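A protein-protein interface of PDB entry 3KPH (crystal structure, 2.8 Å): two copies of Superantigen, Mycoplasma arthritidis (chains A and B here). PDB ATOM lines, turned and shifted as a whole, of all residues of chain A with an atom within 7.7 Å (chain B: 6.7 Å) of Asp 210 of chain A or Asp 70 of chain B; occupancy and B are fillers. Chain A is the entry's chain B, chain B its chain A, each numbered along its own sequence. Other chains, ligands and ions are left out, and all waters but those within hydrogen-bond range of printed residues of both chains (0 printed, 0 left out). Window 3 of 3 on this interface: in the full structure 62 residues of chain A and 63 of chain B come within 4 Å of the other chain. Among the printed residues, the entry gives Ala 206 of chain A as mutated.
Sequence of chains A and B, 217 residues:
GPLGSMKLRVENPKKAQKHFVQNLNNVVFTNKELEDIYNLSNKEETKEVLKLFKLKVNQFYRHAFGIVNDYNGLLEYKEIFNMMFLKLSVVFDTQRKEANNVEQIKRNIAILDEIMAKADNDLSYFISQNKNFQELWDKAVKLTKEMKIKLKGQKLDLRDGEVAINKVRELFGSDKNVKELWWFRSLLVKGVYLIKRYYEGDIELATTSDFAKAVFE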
ATOM      1  N   TRP A 183      -8.936 -15.795 -24.645  1.00  0.00           N
ATOM      2  CA  TRP A 183      -8.769 -14.343 -24.628  1.00  0.00           C
ATOM      3  C   TRP A 183      -9.115 -13.750 -25.998  1.00  0.00           C
ATOM      4  O   TRP A 183     -10.002 -12.910 -26.116  1.00  0.00           O
ATOM      5  CB  TRP A 183      -7.321 -14.031 -24.220  1.00  0.00           C
ATOM      6  CG  TRP A 183      -6.825 -12.649 -24.493  1.00  0.00           C
ATOM      7  CD1 TRP A 183      -5.918 -12.281 -25.445  1.00  0.00           C
ATOM      8  CD2 TRP A 183      -7.135 -11.462 -23.754  1.00  0.00           C
ATOM      9  NE1 TRP A 183      -5.633 -10.941 -25.340  1.00  0.00           N
ATOM     10  CE2 TRP A 183      -6.367 -10.411 -24.311  1.00  0.00           C
ATOM     11  CE3 TRP A 183      -7.983 -11.180 -22.671  1.00  0.00           C
ATOM     12  CZ2 TRP A 183      -6.423  -9.102 -23.822  1.00  0.00           C
ATOM     13  CZ3 TRP A 183      -8.037  -9.875 -22.184  1.00  0.00           C
ATOM     14  CH2 TRP A 183      -7.261  -8.856 -22.761  1.00  0.00           C
ATOM     15  N   SER A 186     -12.838 -14.230 -26.777  1.00  0.00           N
ATOM     16  CA  SER A 186     -13.716 -13.297 -26.077  1.00  0.00           C
ATOM     17  C   SER A 186     -13.743 -11.934 -26.750  1.00  0.00           C
ATOM     18  O   SER A 186     -14.820 -11.333 -26.882  1.00  0.00           O
ATOM     19  CB  SER A 186     -13.275 -13.119 -24.631  1.00  0.00           C
ATOM     20  OG  SER A 186     -12.086 -12.354 -24.590  1.00  0.00           O
ATOM     21  N   LEU A 187     -12.572 -11.441 -27.159  1.00  0.00           N
ATOM     22  CA  LEU A 187     -12.504 -10.143 -27.827  1.00  0.00           C
ATOM     23  C   LEU A 187     -13.231 -10.202 -29.175  1.00  0.00           C
ATOM     24  O   LEU A 187     -14.063  -9.340 -29.482  1.00  0.00           O
ATOM     25  CB  LEU A 187     -11.050  -9.700 -28.042  1.00  0.00           C
ATOM     26  CG  LEU A 187     -10.261  -8.902 -26.985  1.00  0.00           C
ATOM     27  CD1 LEU A 187     -11.158  -8.475 -25.848  1.00  0.00           C
ATOM     28  CD2 LEU A 187      -9.106  -9.713 -26.460  1.00  0.00           C
ATOM     29  N   LYS A 190     -16.937 -10.227 -28.767  1.00  0.00           N
ATOM     30  CA  LYS A 190     -17.323  -8.915 -28.274  1.00  0.00           C
ATOM     31  C   LYS A 190     -17.347  -7.951 -29.448  1.00  0.00           C
ATOM     32  O   LYS A 190     -18.251  -7.126 -29.570  1.00  0.00           O
ATOM     33  CB  LYS A 190     -16.292  -8.474 -27.230  1.00  0.00           C
ATOM     34  CG  LYS A 190     -16.286  -7.015 -26.833  1.00  0.00           C
ATOM     35  CD  LYS A 190     -15.257  -6.783 -25.712  1.00  0.00           C
ATOM     36  CE  LYS A 190     -15.733  -7.346 -24.363  1.00  0.00           C
ATOM     37  NZ  LYS A 190     -16.073  -8.811 -24.355  1.00  0.00           N
ATOM     38  N   LEU A 194     -20.750  -5.913 -30.908  1.00  0.00           N
ATOM     39  CA  LEU A 194     -20.884  -4.476 -30.839  1.00  0.00           C
ATOM     40  C   LEU A 194     -21.057  -3.872 -32.222  1.00  0.00           C
ATOM     41  O   LEU A 194     -21.869  -2.964 -32.400  1.00  0.00           O
ATOM     42  CB  LEU A 194     -19.708  -3.854 -30.075  1.00  0.00           C
ATOM     43  CG  LEU A 194     -18.329  -3.747 -30.691  1.00  0.00           C
ATOM     44  CD1 LEU A 194     -18.347  -2.668 -31.755  1.00  0.00           C
ATOM     45  CD2 LEU A 194     -17.324  -3.395 -29.609  1.00  0.00           C
ATOM     46  N   LEU A 205     -21.574   3.978 -28.185  1.00  0.00           N
ATOM     47  CA  LEU A 205     -20.881   2.740 -27.866  1.00  0.00           C
ATOM     48  C   LEU A 205     -19.397   3.000 -27.683  1.00  0.00           C
ATOM     49  O   LEU A 205     -18.722   2.287 -26.947  1.00  0.00           O
ATOM     50  CB  LEU A 205     -21.102   1.709 -28.974  1.00  0.00           C
ATOM     51  CG  LEU A 205     -22.348   0.835 -28.839  1.00  0.00           C
ATOM     52  CD1 LEU A 205     -23.560   1.692 -28.587  1.00  0.00           C
ATOM     53  CD2 LEU A 205     -22.526   0.014 -30.092  1.00  0.00           C
ATOM     54  N   ALA A 206     -18.895   4.037 -28.342  1.00  0.00           N
ATOM     55  CA  ALA A 206     -17.489   4.390 -28.242  1.00  0.00           C
ATOM     56  C   ALA A 206     -17.025   4.533 -26.787  1.00  0.00           C
ATOM     57  O   ALA A 206     -15.831   4.698 -26.527  1.00  0.00           O
ATOM     58  CB  ALA A 206     -17.231   5.685 -29.007  1.00  0.00           C
ATOM     59  N   THR A 207     -17.962   4.465 -25.841  1.00  0.00           N
ATOM     60  CA  THR A 207     -17.638   4.594 -24.414  1.00  0.00           C
ATOM     61  C   THR A 207     -18.338   3.513 -23.588  1.00  0.00           C
ATOM     62  O   THR A 207     -18.776   3.760 -22.458  1.00  0.00           O
ATOM     63  CB  THR A 207     -18.075   5.968 -23.861  1.00  0.00           C
ATOM     64  OG1 THR A 207     -19.502   6.094 -23.967  1.00  0.00           O
ATOM     65  CG2 THR A 207     -17.394   7.098 -24.635  1.00  0.00           C
ATOM     66  N   THR A 208     -18.439   2.321 -24.166  1.00  0.00           N
ATOM     67  CA  THR A 208     -19.080   1.165 -23.538  1.00  0.00           C
ATOM     68  C   THR A 208     -18.028   0.266 -22.898  1.00  0.00           C
ATOM     69  O   THR A 208     -18.350  -0.598 -22.076  1.00  0.00           O
ATOM     70  CB  THR A 208     -19.828   0.324 -24.605  1.00  0.00           C
ATOM     71  OG1 THR A 208     -20.900   1.096 -25.160  1.00  0.00           O
ATOM     72  CG2 THR A 208     -20.364  -0.977 -24.003  1.00  0.00           C
ATOM     73  N   SER A 209     -16.774   0.468 -23.303  1.00  0.00           N
ATOM     74  CA  SER A 209     -15.642  -0.312 -22.814  1.00  0.00           C
ATOM     75  C   SER A 209     -14.393   0.201 -23.501  1.00  0.00           C
ATOM     76  O   SER A 209     -14.480   0.899 -24.508  1.00  0.00           O
ATOM     77  CB  SER A 209     -15.814  -1.785 -23.157  1.00  0.00           C
ATOM     78  OG  SER A 209     -15.797  -1.967 -24.563  1.00  0.00           O
ATOM     79  N   ASP A 210     -13.230  -0.153 -22.963  1.00  0.00           N
ATOM     80  CA  ASP A 210     -11.965   0.282 -23.541  1.00  0.00           C
ATOM     81  C   ASP A 210     -11.791  -0.312 -24.926  1.00  0.00           C
ATOM     82  O   ASP A 210     -11.149   0.284 -25.791  1.00  0.00           O
ATOM     83  CB  ASP A 210     -10.803  -0.142 -22.648  1.00  0.00           C
ATOM     84  CG  ASP A 210     -10.890   0.462 -21.261  1.00  0.00           C
ATOM     85  OD1 ASP A 210     -10.931   1.713 -21.173  1.00  0.00           O
ATOM     86  OD2 ASP A 210     -10.918  -0.309 -20.266  1.00  0.00           O
ATOM     87  N   PHE A 211     -12.374  -1.493 -25.126  1.00  0.00           N
ATOM     88  CA  PHE A 211     -12.302  -2.185 -26.406  1.00  0.00           C
ATOM     89  C   PHE A 211     -13.083  -1.408 -27.448  1.00  0.00           C
ATOM     90  O   PHE A 211     -12.568  -1.107 -28.516  1.00  0.00           O
ATOM     91  CB  PHE A 211     -12.884  -3.598 -26.293  1.00  0.00           C
ATOM     92  CG  PHE A 211     -12.777  -4.400 -27.565  1.00  0.00           C
ATOM     93  CD1 PHE A 211     -11.528  -4.714 -28.102  1.00  0.00           C
ATOM     94  CD2 PHE A 211     -13.923  -4.830 -28.233  1.00  0.00           C
ATOM     95  CE1 PHE A 211     -11.423  -5.436 -29.277  1.00  0.00           C
ATOM     96  CE2 PHE A 211     -13.825  -5.559 -29.415  1.00  0.00           C
ATOM     97  CZ  PHE A 211     -12.569  -5.860 -29.935  1.00  0.00           C
ATOM     98  N   ALA A 212     -14.332  -1.084 -27.135  1.00  0.00           N
ATOM     99  CA  ALA A 212     -15.168  -0.342 -28.070  1.00  0.00           C
ATOM    100  C   ALA A 212     -14.562   1.024 -28.362  1.00  0.00           C
ATOM    101  O   ALA A 212     -14.640   1.513 -29.486  1.00  0.00           O
ATOM    102  CB  ALA A 212     -16.581  -0.188 -27.515  1.00  0.00           C
ATOM    103  N   LYS A 213     -13.948   1.641 -27.360  1.00  0.00           N
ATOM    104  CA  LYS A 213     -13.349   2.949 -27.577  1.00  0.00           C
ATOM    105  C   LYS A 213     -12.207   2.822 -28.586  1.00  0.00           C
ATOM    106  O   LYS A 213     -12.095   3.638 -29.499  1.00  0.00           O
ATOM    107  CB  LYS A 213     -12.830   3.545 -26.264  1.00  0.00           C
ATOM    108  CG  LYS A 213     -12.342   4.990 -26.388  1.00  0.00           C
ATOM    109  CD  LYS A 213     -11.398   5.350 -25.250  1.00  0.00           C
ATOM    110  CE  LYS A 213     -10.763   6.720 -25.451  1.00  0.00           C
ATOM    111  NZ  LYS A 213      -9.621   6.979 -24.511  1.00  0.00           N
ATOM    112  N   ALA A 214     -11.372   1.798 -28.432  1.00  0.00           N
ATOM    113  CA  ALA A 214     -10.259   1.591 -29.354  1.00  0.00           C
ATOM    114  C   ALA A 214     -10.754   1.186 -30.740  1.00  0.00           C
ATOM    115  O   ALA A 214     -10.120   1.492 -31.745  1.00  0.00           O
ATOM    116  CB  ALA A 214      -9.324   0.538 -28.819  1.00  0.00           C
ATOM    117  N   VAL A 215     -11.890   0.499 -30.788  1.00  0.00           N
ATOM    118  CA  VAL A 215     -12.471   0.056 -32.050  1.00  0.00           C
ATOM    119  C   VAL A 215     -13.072   1.210 -32.838  1.00  0.00           C
ATOM    120  O   VAL A 215     -13.067   1.201 -34.067  1.00  0.00           O
ATOM    121  CB  VAL A 215     -13.563  -1.004 -31.810  1.00  0.00           C
ATOM    122  CG1 VAL A 215     -14.569  -1.003 -32.946  1.00  0.00           C
ATOM    123  CG2 VAL A 215     -12.920  -2.365 -31.689  1.00  0.00           C
ATOM    124  N   PHE A 216     -13.581   2.209 -32.124  1.00  0.00           N
ATOM    125  CA  PHE A 216     -14.205   3.354 -32.768  1.00  0.00           C
ATOM    126  C   PHE A 216     -13.354   4.625 -32.869  1.00  0.00           C
ATOM    127  O   PHE A 216     -13.802   5.617 -33.432  1.00  0.00           O
ATOM    128  CB  PHE A 216     -15.516   3.670 -32.060  1.00  0.00           C
ATOM    129  CG  PHE A 216     -16.581   2.638 -32.265  1.00  0.00           C
ATOM    130  CD1 PHE A 216     -17.375   2.659 -33.402  1.00  0.00           C
ATOM    131  CD2 PHE A 216     -16.813   1.659 -31.308  1.00  0.00           C
ATOM    132  CE1 PHE A 216     -18.397   1.720 -33.584  1.00  0.00           C
ATOM    133  CE2 PHE A 216     -17.830   0.713 -31.476  1.00  0.00           C
ATOM    134  CZ  PHE A 216     -18.625   0.745 -32.618  1.00  0.00           C
ATOM    135  N   PHE B  65     -16.946  -2.583 -13.056  1.00  0.00           N
ATOM    136  CA  PHE B  65     -17.672  -3.328 -14.071  1.00  0.00           C
ATOM    137  C   PHE B  65     -17.020  -3.194 -15.431  1.00  0.00           C
ATOM    138  O   PHE B  65     -17.172  -4.063 -16.286  1.00  0.00           O
ATOM    139  CB  PHE B  65     -19.135  -2.895 -14.112  1.00  0.00           C
ATOM    140  CG  PHE B  65     -19.931  -3.389 -12.936  1.00  0.00           C
ATOM    141  CD1 PHE B  65     -20.037  -2.625 -11.780  1.00  0.00           C
ATOM    142  CD2 PHE B  65     -20.531  -4.648 -12.968  1.00  0.00           C
ATOM    143  CE1 PHE B  65     -20.727  -3.110 -10.666  1.00  0.00           C
ATOM    144  CE2 PHE B  65     -21.222  -5.143 -11.861  1.00  0.00           C
ATOM    145  CZ  PHE B  65     -21.320  -4.372 -10.708  1.00  0.00           C
ATOM    146  N   GLY B  66     -16.280  -2.112 -15.628  1.00  0.00           N
ATOM    147  CA  GLY B  66     -15.592  -1.948 -16.889  1.00  0.00           C
ATOM    148  C   GLY B  66     -14.718  -3.180 -17.023  1.00  0.00           C
ATOM    149  O   GLY B  66     -14.700  -3.838 -18.060  1.00  0.00           O
ATOM    150  N   ILE B  67     -14.014  -3.514 -15.946  1.00  0.00           N
ATOM    151  CA  ILE B  67     -13.130  -4.675 -15.947  1.00  0.00           C
ATOM    152  C   ILE B  67     -13.868  -5.969 -16.242  1.00  0.00           C
ATOM    153  O   ILE B  67     -13.350  -6.826 -16.949  1.00  0.00           O
ATOM    154  CB  ILE B  67     -12.408  -4.867 -14.589  1.00  0.00           C
ATOM    155  CG1 ILE B  67     -11.597  -3.620 -14.240  1.00  0.00           C
ATOM    156  CG2 ILE B  67     -11.498  -6.087 -14.664  1.00  0.00           C
ATOM    157  CD1 ILE B  67     -10.997  -3.661 -12.861  1.00  0.00           C
ATOM    158  N   VAL B  68     -15.076  -6.114 -15.707  1.00  0.00           N
ATOM    159  CA  VAL B  68     -15.833  -7.342 -15.908  1.00  0.00           C
ATOM    160  C   VAL B  68     -16.439  -7.509 -17.288  1.00  0.00           C
ATOM    161  O   VAL B  68     -16.937  -8.578 -17.607  1.00  0.00           O
ATOM    162  CB  VAL B  68     -16.964  -7.479 -14.883  1.00  0.00           C
ATOM    163  CG1 VAL B  68     -17.606  -8.843 -14.991  1.00  0.00           C
ATOM    164  CG2 VAL B  68     -16.421  -7.288 -13.511  1.00  0.00           C
ATOM    165  N   ASN B  69     -16.398  -6.475 -18.117  1.00  0.00           N
ATOM    166  CA  ASN B  69     -16.990  -6.599 -19.448  1.00  0.00           C
ATOM    167  C   ASN B  69     -16.067  -6.085 -20.531  1.00  0.00           C
ATOM    168  O   ASN B  69     -16.502  -5.719 -21.621  1.00  0.00           O
ATOM    169  CB  ASN B  69     -18.328  -5.833 -19.510  1.00  0.00           C
ATOM    170  CG  ASN B  69     -18.152  -4.312 -19.698  1.00  0.00           C
ATOM    171  OD1 ASN B  69     -19.129  -3.558 -19.634  1.00  0.00           O
ATOM    172  ND2 ASN B  69     -16.917  -3.863 -19.940  1.00  0.00           N
ATOM    173  N   ASP B  70     -14.784  -6.063 -20.227  1.00  0.00           N
ATOM    174  CA  ASP B  70     -13.806  -5.557 -21.165  1.00  0.00           C
ATOM    175  C   ASP B  70     -12.547  -6.396 -20.948  1.00  0.00           C
ATOM    176  O   ASP B  70     -11.546  -6.233 -21.639  1.00  0.00           O
ATOM    177  CB  ASP B  70     -13.579  -4.078 -20.835  1.00  0.00           C
ATOM    178  CG  ASP B  70     -12.894  -3.329 -21.931  1.00  0.00           C
ATOM    179  OD1 ASP B  70     -13.353  -3.415 -23.084  1.00  0.00           O
ATOM    180  OD2 ASP B  70     -11.902  -2.638 -21.630  1.00  0.00           O
ATOM    181  N   TYR B  71     -12.621  -7.311 -19.983  1.00  0.00           N
ATOM    182  CA  TYR B  71     -11.490  -8.161 -19.649  1.00  0.00           C
ATOM    183  C   TYR B  71     -11.891  -9.545 -19.173  1.00  0.00           C
ATOM    184  O   TYR B  71     -11.077 -10.270 -18.608  1.00  0.00           O
ATOM    185  CB  TYR B  71     -10.630  -7.471 -18.593  1.00  0.00           C
ATOM    186  CG  TYR B  71      -9.856  -6.323 -19.167  1.00  0.00           C
ATOM    187  CD1 TYR B  71      -8.718  -6.553 -19.928  1.00  0.00           C
ATOM    188  CD2 TYR B  71     -10.307  -5.015 -19.032  1.00  0.00           C
ATOM    189  CE1 TYR B  71      -8.047  -5.515 -20.551  1.00  0.00           C
ATOM    190  CE2 TYR B  71      -9.645  -3.962 -19.654  1.00  0.00           C
ATOM    191  CZ  TYR B  71      -8.512  -4.222 -20.416  1.00  0.00           C
ATOM    192  OH  TYR B  71      -7.841  -3.200 -21.056  1.00  0.00           O
ATOM    193  N   ASN B  72     -13.143  -9.917 -19.413  1.00  0.00           N
ATOM    194  CA  ASN B  72     -13.628 -11.237 -19.019  1.00  0.00           C
ATOM    195  C   ASN B  72     -12.856 -12.340 -19.747  1.00  0.00           C
ATOM    196  O   ASN B  72     -12.988 -13.523 -19.432  1.00  0.00           O
ATOM    197  CB  ASN B  72     -15.112 -11.378 -19.338  1.00  0.00           C
ATOM    198  CG  ASN B  72     -15.412 -11.109 -20.791  1.00  0.00           C
ATOM    199  OD1 ASN B  72     -15.312  -9.975 -21.253  1.00  0.00           O
ATOM    200  ND2 ASN B  72     -15.768 -12.152 -21.529  1.00  0.00           N
ATOM    201  N   GLY B  73     -12.063 -11.960 -20.740  1.00  0.00           N
ATOM    202  CA  GLY B  73     -11.295 -12.955 -21.460  1.00  0.00           C
ATOM    203  C   GLY B  73     -10.066 -13.302 -20.652  1.00  0.00           C
ATOM    204  O   GLY B  73      -9.413 -14.313 -20.895  1.00  0.00           O
ATOM    205  N   LEU B 123      -4.335  -5.768 -13.663  1.00  0.00           N
ATOM    206  CA  LEU B 123      -4.777  -6.013 -15.022  1.00  0.00           C
ATOM    207  C   LEU B 123      -3.593  -5.996 -15.987  1.00  0.00           C
ATOM    208  O   LEU B 123      -3.530  -6.787 -16.926  1.00  0.00           O
ATOM    209  CB  LEU B 123      -5.774  -4.942 -15.415  1.00  0.00           C
ATOM    210  CG  LEU B 123      -7.123  -5.386 -15.951  1.00  0.00           C
ATOM    211  CD1 LEU B 123      -7.772  -6.381 -15.006  1.00  0.00           C
ATOM    212  CD2 LEU B 123      -7.990  -4.140 -16.134  1.00  0.00           C
ATOM    213  N   TRP B 137      -4.986  -8.746 -28.582  1.00  0.00           N
ATOM    214  CA  TRP B 137      -5.936  -7.655 -28.337  1.00  0.00           C
ATOM    215  C   TRP B 137      -5.920  -6.701 -29.535  1.00  0.00           C
ATOM    216  O   TRP B 137      -6.959  -6.390 -30.116  1.00  0.00           O
ATOM    217  CB  TRP B 137      -5.560  -6.897 -27.051  1.00  0.00           C
ATOM    218  CG  TRP B 137      -6.256  -5.556 -26.866  1.00  0.00           C
ATOM    219  CD1 TRP B 137      -5.879  -4.359 -27.402  1.00  0.00           C
ATOM    220  CD2 TRP B 137      -7.433  -5.292 -26.089  1.00  0.00           C
ATOM    221  NE1 TRP B 137      -6.744  -3.367 -27.006  1.00  0.00           N
ATOM    222  CE2 TRP B 137      -7.707  -3.911 -26.201  1.00  0.00           C
ATOM    223  CE3 TRP B 137      -8.282  -6.087 -25.311  1.00  0.00           C
ATOM    224  CZ2 TRP B 137      -8.794  -3.305 -25.564  1.00  0.00           C
ATOM    225  CZ3 TRP B 137      -9.366  -5.483 -24.675  1.00  0.00           C
ATOM    226  CH2 TRP B 137      -9.611  -4.103 -24.808  1.00  0.00           C
ATOM    227  N   VAL B 141      -8.897  -5.886 -32.171  1.00  0.00           N
ATOM    228  CA  VAL B 141      -9.319  -4.505 -32.417  1.00  0.00           C
ATOM    229  C   VAL B 141      -9.275  -4.256 -33.923  1.00  0.00           C
ATOM    230  O   VAL B 141     -10.252  -3.777 -34.509  1.00  0.00           O
ATOM    231  CB  VAL B 141      -8.382  -3.476 -31.741  1.00  0.00           C
ATOM    232  CG1 VAL B 141      -8.807  -2.069 -32.119  1.00  0.00           C
ATOM    233  CG2 VAL B 141      -8.418  -3.640 -30.236  1.00  0.00           C
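Tyr 71 of chain B touches Trp 183 of chain A (CD1 to CH2, 3.9 Å). Trp 183 of chain A touches Gly 73 of chain B. Trp 183 of chain A touches Trp 137 of chain B (CZ2 to CE3, 3.8 Å). OG of Ser 186 of chain A touches CA of Gly 73 of chain B (3.3 Å). CE of Lys 190 of chain A touches O of Asn 69 of chain B, 3.3 Å away. Asn 69 of chain B touches Thr 208 of chain A (OD1 to O, 3.9 Å). CB of Ser 209 of chain A touches ND2 of Asn 69 of chain B (3.99 Å). OD2 of Asp 210 of chain A touches CE2 of Tyr 71 of chain B, 3.9 Å away. Phe 211 of chain A touches Trp 137 of chain B. CG1 of Val 141 of chain B touches O of Ala 214 of chain A, 3.8 Å away.
The side-chain carboxylate of Asp 70 of chain B lies close to the side-chain hydroxyl of Ser 209 of chain A (3.2 Å). N of Asp 210 of chain A lies close to OD2 of Asp 70 of chain B (3.1 Å). OD1 of Asp 70 of chain B is in hydrogen-bond range of N of Phe 211 of chain A (3.0 Å). The side-chain amino group of Lys 190 of chain A sits at hydrogen-bond distance from the side-chain amide oxygen of Asn 72 of chain B.
No position is printed for both chains.
ND2 of Asn 69 of chain B lies within hydrogen-bond range of O of Gly 66 of chain B (2.9 Å). O of Trp 183 of chain A is in hydrogen-bond range of OG of Ser 186 of chain A, 2.6 Å away. O of Leu 205 of chain A lies within hydrogen-bond range of OG1 of Thr 208 of chain A, 3.1 Å away. The backbone NH (N) of Ala 212 of chain A is in hydrogen-bond range of the side-chain hydroxyl (OG) of Ser 209 of chain A, at 3.1 Å.
Hydrophobic or aromatic side chains of chain B that line the printed part of chain A: Tyr 71, Trp 137 and Val 141. Of the 17 printed residues of chain A, 9 touch a printed residue of chain B. Hydrophobic or aromatic side chains of chain A within 4 Å of the printed part of chain B: Trp 183, Leu 187 and Phe 211. Among the printed residues, no Asp or Glu carboxylate lies within 4 Å of a Lys or Arg side-chain nitrogen of the other chain.
Asp 210 of chain A touches just these residues of chain B: Asp 70 and Tyr 71. Of chain A, only Ser 209 (3.0 Å), Asp 210 (2.9 Å) and Phe 211 (3.0 Å) come within 4 Å of Asp 70 of chain B. Of the printed residues of chain A, Val 141 of chain B touches Phe 211 (3.6 Å) and Ala 214 (3.8 Å). Printed residues of chain B within 4 Å of Ser 209 of chain A: Asn 69 and Asp 70. Leu 123 of chain B touches none of the printed residues of chain A. Leu 194 of chain A touches none of the printed residues of chain B. The nearest residue of chain B that does not touch Asp 210 of chain A is Trp 137 of chain B (4.3 Å).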
